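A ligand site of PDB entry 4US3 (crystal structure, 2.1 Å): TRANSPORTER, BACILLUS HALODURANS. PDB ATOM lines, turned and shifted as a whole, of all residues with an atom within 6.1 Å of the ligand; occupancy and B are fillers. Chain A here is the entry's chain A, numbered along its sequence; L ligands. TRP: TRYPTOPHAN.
N of Gly 32 is in hydrogen-bond range of O of the ligand, at 2.7 Å. OH of Tyr 110 lies within hydrogen-bond range of O of the ligand (2.8 Å). The side-chain hydroxyl of Ser 235 lies within hydrogen-bond range of a nitrogen (N) of the ligand (2.8 Å). A nitrogen (NE1) of the ligand sits at hydrogen-bond distance from the side-chain hydroxyl (OG) of Ser 329 (3.0 Å). The backbone carbonyl oxygen (O) of Ala 28 is in hydrogen-bond range of a nitrogen (N) of the ligand (3.0 Å). The backbone carbonyl oxygen (O) of Phe 232 lies within hydrogen-bond range of a nitrogen (N) of the ligand (3.0 Å). The backbone NH (N) of Leu 31 sits at hydrogen-bond distance from an oxygen (O) of the ligand. The backbone carbonyl oxygen of Thr 233 sits at hydrogen-bond distance from a nitrogen (N) of the ligand (3.3 Å). O of Ser 27 lies close to N of the ligand, at 3.4 Å.
Merely in contact with the ligand: Gly 30 (3.5 Å), Asn 33 (3.6 Å), Leu 236 (3.8 Å), Met 238 (3.4 Å), Ala 240 (3.8 Å), Ser 326 (3.4 Å), Leu 330 (3.5 Å) and Leu 395 (3.9 Å). Hydrophobic or aromatic side chains that line the ligand: Tyr 110, Phe 232, Met 238, Ala 240, Leu 330 and Leu 395. 17 residues have an atom within 4 Å of the ligand: Ser 27, Ala 28, Gly 30, Leu 31, Gly 32, Asn 33, Tyr 110, Phe 232, Thr 233, Ser 235, Leu 236, Met 238, Ala 240, Ser 326, Ser 329, Leu 330 and Leu 395.
N of Leu 31 lies within hydrogen-bond range of OH of Tyr 110, 3.0 Å away. OG of Ser 235 sits close to N of Ala 28 (3.4 Å). The side-chain hydroxyl (OG) of Ser 235 sits at hydrogen-bond distance from the side-chain hydroxyl (OG) of Ser 27, 2.8 Å away. OG of Ser 329 is in hydrogen-bond range of OG of Ser 27, at 2.9 Å. The side-chain hydroxyl (OG1) of Thr 233 sits at hydrogen-bond distance from the side-chain carboxylate (OD2) of Asp 265, at 2.7 Å. O of Ser 27 sits at hydrogen-bond distance from OG of Ser 326 (2.9 Å). The side-chain amide oxygen (OD1) of Asn 33 lies within hydrogen-bond range of the backbone NH (N) of Gly 30, at 3.0 Å. The side-chain carboxylate of Asp 265 is in hydrogen-bond range of the side-chain amide nitrogen of Asn 33 (2.7 Å).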
ATOM      1  N   SER A  27      11.246   6.426  -0.443  1.00  0.00           N
ATOM      2  CA  SER A  27      10.072   5.879   0.205  1.00  0.00           C
ATOM      3  C   SER A  27       9.718   4.509  -0.330  1.00  0.00           C
ATOM      4  O   SER A  27       9.485   3.565   0.438  1.00  0.00           O
ATOM      5  CB  SER A  27       8.870   6.795  -0.008  1.00  0.00           C
ATOM      6  OG  SER A  27       7.676   6.167   0.437  1.00  0.00           O
ATOM      7  N   ALA A  28       9.700   4.404  -1.655  1.00  0.00           N
ATOM      8  CA  ALA A  28       9.218   3.213  -2.321  1.00  0.00           C
ATOM      9  C   ALA A  28      10.139   2.003  -2.173  1.00  0.00           C
ATOM     10  O   ALA A  28       9.657   0.897  -1.974  1.00  0.00           O
ATOM     11  CB  ALA A  28       8.987   3.494  -3.818  1.00  0.00           C
ATOM     12  N   VAL A  29      11.446   2.216  -2.345  1.00  0.00           N
ATOM     13  CA  VAL A  29      12.393   1.105  -2.370  1.00  0.00           C
ATOM     14  C   VAL A  29      12.895   0.760  -0.961  1.00  0.00           C
ATOM     15  O   VAL A  29      13.502   1.596  -0.299  1.00  0.00           O
ATOM     16  CB  VAL A  29      13.593   1.417  -3.297  1.00  0.00           C
ATOM     17  CG1 VAL A  29      14.639   0.342  -3.185  1.00  0.00           C
ATOM     18  CG2 VAL A  29      13.143   1.570  -4.752  1.00  0.00           C
ATOM     19  N   GLY A  30      12.612  -0.469  -0.525  1.00  0.00           N
ATOM     20  CA  GLY A  30      13.001  -0.945   0.789  1.00  0.00           C
ATOM     21  C   GLY A  30      12.661  -2.417   0.994  1.00  0.00           C
ATOM     22  O   GLY A  30      12.748  -3.245   0.066  1.00  0.00           O
ATOM     23  N   LEU A  31      12.234  -2.748   2.213  1.00  0.00           N
ATOM     24  CA  LEU A  31      11.943  -4.134   2.589  1.00  0.00           C
ATOM     25  C   LEU A  31      10.886  -4.791   1.699  1.00  0.00           C
ATOM     26  O   LEU A  31      10.916  -6.008   1.498  1.00  0.00           O
ATOM     27  CB  LEU A  31      11.516  -4.204   4.063  1.00  0.00           C
ATOM     28  CG  LEU A  31      12.539  -3.825   5.151  1.00  0.00           C
ATOM     29  CD1 LEU A  31      11.919  -3.955   6.557  1.00  0.00           C
ATOM     30  CD2 LEU A  31      13.806  -4.650   5.053  1.00  0.00           C
ATOM     31  N   GLY A  32       9.949  -4.003   1.188  1.00  0.00           N
ATOM     32  CA  GLY A  32       8.895  -4.553   0.363  1.00  0.00           C
ATOM     33  C   GLY A  32       9.428  -5.159  -0.926  1.00  0.00           C
ATOM     34  O   GLY A  32       8.813  -6.054  -1.491  1.00  0.00           O
ATOM     35  N   ASN A  33      10.578  -4.679  -1.383  1.00  0.00           N
ATOM     36  CA  ASN A  33      11.164  -5.135  -2.633  1.00  0.00           C
ATOM     37  C   ASN A  33      11.938  -6.433  -2.491  1.00  0.00           C
ATOM     38  O   ASN A  33      12.082  -7.180  -3.458  1.00  0.00           O
ATOM     39  CB  ASN A  33      12.138  -4.095  -3.191  1.00  0.00           C
ATOM     40  CG  ASN A  33      11.465  -2.788  -3.544  1.00  0.00           C
ATOM     41  OD1 ASN A  33      11.174  -1.987  -2.661  1.00  0.00           O
ATOM     42  ND2 ASN A  33      11.223  -2.565  -4.833  1.00  0.00           N
ATOM     43  N   ILE A 106       1.271  -0.346   9.626  1.00  0.00           N
ATOM     44  CA  ILE A 106       2.362  -0.861   8.807  1.00  0.00           C
ATOM     45  C   ILE A 106       3.721  -0.649   9.481  1.00  0.00           C
ATOM     46  O   ILE A 106       4.507  -1.580   9.583  1.00  0.00           O
ATOM     47  CB  ILE A 106       2.347  -0.311   7.368  1.00  0.00           C
ATOM     48  CG1 ILE A 106       1.113  -0.832   6.649  1.00  0.00           C
ATOM     49  CG2 ILE A 106       3.611  -0.783   6.633  1.00  0.00           C
ATOM     50  CD1 ILE A 106       0.886  -0.226   5.273  1.00  0.00           C
ATOM     51  N   TYR A 110       6.855  -3.142  10.303  1.00  0.00           N
ATOM     52  CA  TYR A 110       7.994  -2.786   9.450  1.00  0.00           C
ATOM     53  C   TYR A 110       9.238  -2.613  10.321  1.00  0.00           C
ATOM     54  O   TYR A 110      10.332  -3.076   9.974  1.00  0.00           O
ATOM     55  CB  TYR A 110       7.702  -1.502   8.673  1.00  0.00           C
ATOM     56  CG  TYR A 110       8.544  -1.303   7.429  1.00  0.00           C
ATOM     57  CD1 TYR A 110       9.772  -0.623   7.482  1.00  0.00           C
ATOM     58  CD2 TYR A 110       8.102  -1.752   6.199  1.00  0.00           C
ATOM     59  CE1 TYR A 110      10.544  -0.438   6.329  1.00  0.00           C
ATOM     60  CE2 TYR A 110       8.865  -1.557   5.040  1.00  0.00           C
ATOM     61  CZ  TYR A 110      10.095  -0.905   5.110  1.00  0.00           C
ATOM     62  OH  TYR A 110      10.825  -0.738   3.949  1.00  0.00           O
ATOM     63  N   GLN A 229       0.645  -6.260  -2.525  1.00  0.00           N
ATOM     64  CA  GLN A 229       2.076  -6.134  -2.744  1.00  0.00           C
ATOM     65  C   GLN A 229       2.360  -4.971  -3.681  1.00  0.00           C
ATOM     66  O   GLN A 229       3.344  -4.275  -3.507  1.00  0.00           O
ATOM     67  CB  GLN A 229       2.678  -7.422  -3.285  1.00  0.00           C
ATOM     68  CG  GLN A 229       4.150  -7.333  -3.626  1.00  0.00           C
ATOM     69  CD  GLN A 229       5.034  -7.119  -2.414  1.00  0.00           C
ATOM     70  OE1 GLN A 229       4.684  -7.519  -1.303  1.00  0.00           O
ATOM     71  NE2 GLN A 229       6.193  -6.471  -2.619  1.00  0.00           N
ATOM     72  N   PHE A 231       0.454  -2.182  -4.001  1.00  0.00           N
ATOM     73  CA  PHE A 231       0.290  -0.993  -3.160  1.00  0.00           C
ATOM     74  C   PHE A 231       1.425  -0.832  -2.127  1.00  0.00           C
ATOM     75  O   PHE A 231       1.991   0.254  -1.971  1.00  0.00           O
ATOM     76  CB  PHE A 231      -1.071  -1.000  -2.444  1.00  0.00           C
ATOM     77  CG  PHE A 231      -2.219  -0.504  -3.303  1.00  0.00           C
ATOM     78  CD1 PHE A 231      -2.448   0.856  -3.445  1.00  0.00           C
ATOM     79  CD2 PHE A 231      -3.042  -1.390  -3.966  1.00  0.00           C
ATOM     80  CE1 PHE A 231      -3.492   1.319  -4.244  1.00  0.00           C
ATOM     81  CE2 PHE A 231      -4.091  -0.926  -4.757  1.00  0.00           C
ATOM     82  CZ  PHE A 231      -4.307   0.422  -4.902  1.00  0.00           C
ATOM     83  N   PHE A 232       1.728  -1.914  -1.421  1.00  0.00           N
ATOM     84  CA  PHE A 232       2.776  -1.888  -0.402  1.00  0.00           C
ATOM     85  C   PHE A 232       4.098  -1.381  -1.012  1.00  0.00           C
ATOM     86  O   PHE A 232       4.659  -0.410  -0.533  1.00  0.00           O
ATOM     87  CB  PHE A 232       2.949  -3.287   0.252  1.00  0.00           C
ATOM     88  CG  PHE A 232       3.812  -3.288   1.511  1.00  0.00           C
ATOM     89  CD1 PHE A 232       5.211  -3.285   1.430  1.00  0.00           C
ATOM     90  CD2 PHE A 232       3.225  -3.295   2.777  1.00  0.00           C
ATOM     91  CE1 PHE A 232       6.015  -3.282   2.589  1.00  0.00           C
ATOM     92  CE2 PHE A 232       4.000  -3.309   3.946  1.00  0.00           C
ATOM     93  CZ  PHE A 232       5.403  -3.307   3.857  1.00  0.00           C
ATOM     94  N   THR A 233       4.533  -2.016  -2.096  1.00  0.00           N
ATOM     95  CA  THR A 233       5.850  -1.706  -2.667  1.00  0.00           C
ATOM     96  C   THR A 233       5.956  -0.282  -3.225  1.00  0.00           C
ATOM     97  O   THR A 233       7.039   0.322  -3.246  1.00  0.00           O
ATOM     98  CB  THR A 233       6.252  -2.761  -3.736  1.00  0.00           C
ATOM     99  OG1 THR A 233       7.666  -2.698  -3.989  1.00  0.00           O
ATOM    100  CG2 THR A 233       5.485  -2.551  -5.034  1.00  0.00           C
ATOM    101  N   LEU A 234       4.816   0.262  -3.644  1.00  0.00           N
ATOM    102  CA  LEU A 234       4.752   1.600  -4.208  1.00  0.00           C
ATOM    103  C   LEU A 234       4.543   2.695  -3.159  1.00  0.00           C
ATOM    104  O   LEU A 234       4.410   3.870  -3.517  1.00  0.00           O
ATOM    105  CB  LEU A 234       3.640   1.696  -5.269  1.00  0.00           C
ATOM    106  CG  LEU A 234       3.926   0.978  -6.589  1.00  0.00           C
ATOM    107  CD1 LEU A 234       2.893   1.299  -7.656  1.00  0.00           C
ATOM    108  CD2 LEU A 234       5.334   1.330  -7.073  1.00  0.00           C
ATOM    109  N   SER A 235       4.554   2.311  -1.874  1.00  0.00           N
ATOM    110  CA  SER A 235       4.273   3.227  -0.765  1.00  0.00           C
ATOM    111  C   SER A 235       2.918   3.884  -0.983  1.00  0.00           C
ATOM    112  O   SER A 235       2.759   5.100  -0.815  1.00  0.00           O
ATOM    113  CB  SER A 235       5.355   4.305  -0.623  1.00  0.00           C
ATOM    114  OG  SER A 235       6.615   3.715  -0.329  1.00  0.00           O
ATOM    115  N   LEU A 236       1.937   3.064  -1.364  1.00  0.00           N
ATOM    116  CA  LEU A 236       0.743   3.597  -2.025  1.00  0.00           C
ATOM    117  C   LEU A 236      -0.579   3.376  -1.289  1.00  0.00           C
ATOM    118  O   LEU A 236      -0.817   2.333  -0.689  1.00  0.00           O
ATOM    119  CB  LEU A 236       0.649   2.975  -3.433  1.00  0.00           C
ATOM    120  CG  LEU A 236      -0.363   3.609  -4.390  1.00  0.00           C
ATOM    121  CD1 LEU A 236      -0.102   5.090  -4.490  1.00  0.00           C
ATOM    122  CD2 LEU A 236      -0.281   2.954  -5.770  1.00  0.00           C
ATOM    123  N   GLY A 237      -1.452   4.378  -1.368  1.00  0.00           N
ATOM    124  CA  GLY A 237      -2.815   4.246  -0.872  1.00  0.00           C
ATOM    125  C   GLY A 237      -3.065   4.777   0.518  1.00  0.00           C
ATOM    126  O   GLY A 237      -4.207   4.732   0.989  1.00  0.00           O
ATOM    127  N   MET A 238      -2.026   5.271   1.197  1.00  0.00           N
ATOM    128  CA  MET A 238      -2.203   5.751   2.554  1.00  0.00           C
ATOM    129  C   MET A 238      -1.950   7.257   2.686  1.00  0.00           C
ATOM    130  O   MET A 238      -2.073   7.823   3.773  1.00  0.00           O
ATOM    131  CB  MET A 238      -1.289   4.987   3.539  1.00  0.00           C
ATOM    132  CG  MET A 238       0.160   5.538   3.614  1.00  0.00           C
ATOM    133  SD  MET A 238       1.021   5.082   5.149  1.00  0.00           S
ATOM    134  CE  MET A 238       0.703   3.310   5.208  1.00  0.00           C
ATOM    135  N   ALA A 240       1.051   8.601   1.906  1.00  0.00           N
ATOM    136  CA  ALA A 240       2.491   8.828   2.063  1.00  0.00           C
ATOM    137  C   ALA A 240       3.070   9.667   0.910  1.00  0.00           C
ATOM    138  O   ALA A 240       3.952  10.487   1.114  1.00  0.00           O
ATOM    139  CB  ALA A 240       3.251   7.521   2.210  1.00  0.00           C
ATOM    140  N   ASP A 265      11.268   0.936  -8.770  1.00  0.00           N
ATOM    141  CA  ASP A 265      10.842   0.018  -7.742  1.00  0.00           C
ATOM    142  C   ASP A 265      10.630  -1.389  -8.312  1.00  0.00           C
ATOM    143  O   ASP A 265      10.933  -2.397  -7.664  1.00  0.00           O
ATOM    144  CB  ASP A 265       9.567   0.503  -7.071  1.00  0.00           C
ATOM    145  CG  ASP A 265       9.126  -0.413  -5.948  1.00  0.00           C
ATOM    146  OD1 ASP A 265       9.740  -0.338  -4.855  1.00  0.00           O
ATOM    147  OD2 ASP A 265       8.204  -1.232  -6.184  1.00  0.00           O
ATOM    148  N   SER A 325      14.880   4.790   5.069  1.00  0.00           N
ATOM    149  CA  SER A 325      14.229   5.835   4.291  1.00  0.00           C
ATOM    150  C   SER A 325      12.749   5.516   4.095  1.00  0.00           C
ATOM    151  O   SER A 325      11.930   6.424   4.036  1.00  0.00           O
ATOM    152  CB  SER A 325      14.923   6.056   2.943  1.00  0.00           C
ATOM    153  OG  SER A 325      15.200   4.827   2.292  1.00  0.00           O
ATOM    154  N   SER A 326      12.403   4.235   4.004  1.00  0.00           N
ATOM    155  CA  SER A 326      11.010   3.839   3.831  1.00  0.00           C
ATOM    156  C   SER A 326      10.238   4.036   5.140  1.00  0.00           C
ATOM    157  O   SER A 326       9.113   4.511   5.116  1.00  0.00           O
ATOM    158  CB  SER A 326      10.877   2.383   3.344  1.00  0.00           C
ATOM    159  OG  SER A 326      11.497   2.195   2.068  1.00  0.00           O
ATOM    160  N   ALA A 327      10.846   3.648   6.258  1.00  0.00           N
ATOM    161  CA  ALA A 327      10.243   3.841   7.587  1.00  0.00           C
ATOM    162  C   ALA A 327       9.945   5.308   7.905  1.00  0.00           C
ATOM    163  O   ALA A 327       8.904   5.621   8.486  1.00  0.00           O
ATOM    164  CB  ALA A 327      11.139   3.251   8.660  1.00  0.00           C
ATOM    165  N   SER A 329       9.272   7.689   5.753  1.00  0.00           N
ATOM    166  CA  SER A 329       8.092   8.110   5.014  1.00  0.00           C
ATOM    167  C   SER A 329       6.796   7.605   5.661  1.00  0.00           C
ATOM    168  O   SER A 329       5.790   8.292   5.642  1.00  0.00           O
ATOM    169  CB  SER A 329       8.181   7.706   3.531  1.00  0.00           C
ATOM    170  OG  SER A 329       7.699   6.394   3.329  1.00  0.00           O
ATOM    171  N   LEU A 330       6.841   6.413   6.249  1.00  0.00           N
ATOM    172  CA  LEU A 330       5.686   5.895   6.993  1.00  0.00           C
ATOM    173  C   LEU A 330       5.377   6.738   8.236  1.00  0.00           C
ATOM    174  O   LEU A 330       4.214   7.058   8.513  1.00  0.00           O
ATOM    175  CB  LEU A 330       5.913   4.445   7.411  1.00  0.00           C
ATOM    176  CG  LEU A 330       5.761   3.289   6.422  1.00  0.00           C
ATOM    177  CD1 LEU A 330       6.408   2.038   6.981  1.00  0.00           C
ATOM    178  CD2 LEU A 330       4.289   3.029   6.130  1.00  0.00           C
ATOM    179  N   LEU A 395      -4.959  -0.174   2.311  1.00  0.00           N
ATOM    180  CA  LEU A 395      -4.226   0.379   1.170  1.00  0.00           C
ATOM    181  C   LEU A 395      -5.005   0.357  -0.143  1.00  0.00           C
ATOM    182  O   LEU A 395      -5.105   1.376  -0.789  1.00  0.00           O
ATOM    183  CB  LEU A 395      -2.838  -0.265   0.982  1.00  0.00           C
ATOM    184  CG  LEU A 395      -1.777  -0.109   2.091  1.00  0.00           C
ATOM    185  CD1 LEU A 395      -0.455  -0.670   1.605  1.00  0.00           C
ATOM    186  CD2 LEU A 395      -1.629   1.350   2.528  1.00  0.00           C
HETATM  187  N   TRP L   1       7.308   1.003  -0.061  1.00  0.00           N
HETATM  188  CA  TRP L   1       8.161   0.541   1.038  1.00  0.00           C
HETATM  189  C   TRP L   1       8.714  -0.861   0.797  1.00  0.00           C
HETATM  190  O   TRP L   1       9.405  -1.392   1.685  1.00  0.00           O
HETATM  191  CB  TRP L   1       7.415   0.588   2.395  1.00  0.00           C
HETATM  192  CG  TRP L   1       6.591   1.817   2.579  1.00  0.00           C
HETATM  193  CD1 TRP L   1       7.044   3.081   2.876  1.00  0.00           C
HETATM  194  CD2 TRP L   1       5.165   1.915   2.459  1.00  0.00           C
HETATM  195  NE1 TRP L   1       5.975   3.955   2.944  1.00  0.00           N
HETATM  196  CE2 TRP L   1       4.815   3.265   2.676  1.00  0.00           C
HETATM  197  CE3 TRP L   1       4.151   0.996   2.156  1.00  0.00           C
HETATM  198  CZ2 TRP L   1       3.486   3.716   2.630  1.00  0.00           C
HETATM  199  CZ3 TRP L   1       2.831   1.437   2.116  1.00  0.00           C
HETATM  200  CH2 TRP L   1       2.521   2.794   2.342  1.00  0.00           C
HETATM  201  OXT TRP L   1       8.492  -1.462  -0.259  1.00  0.00           O
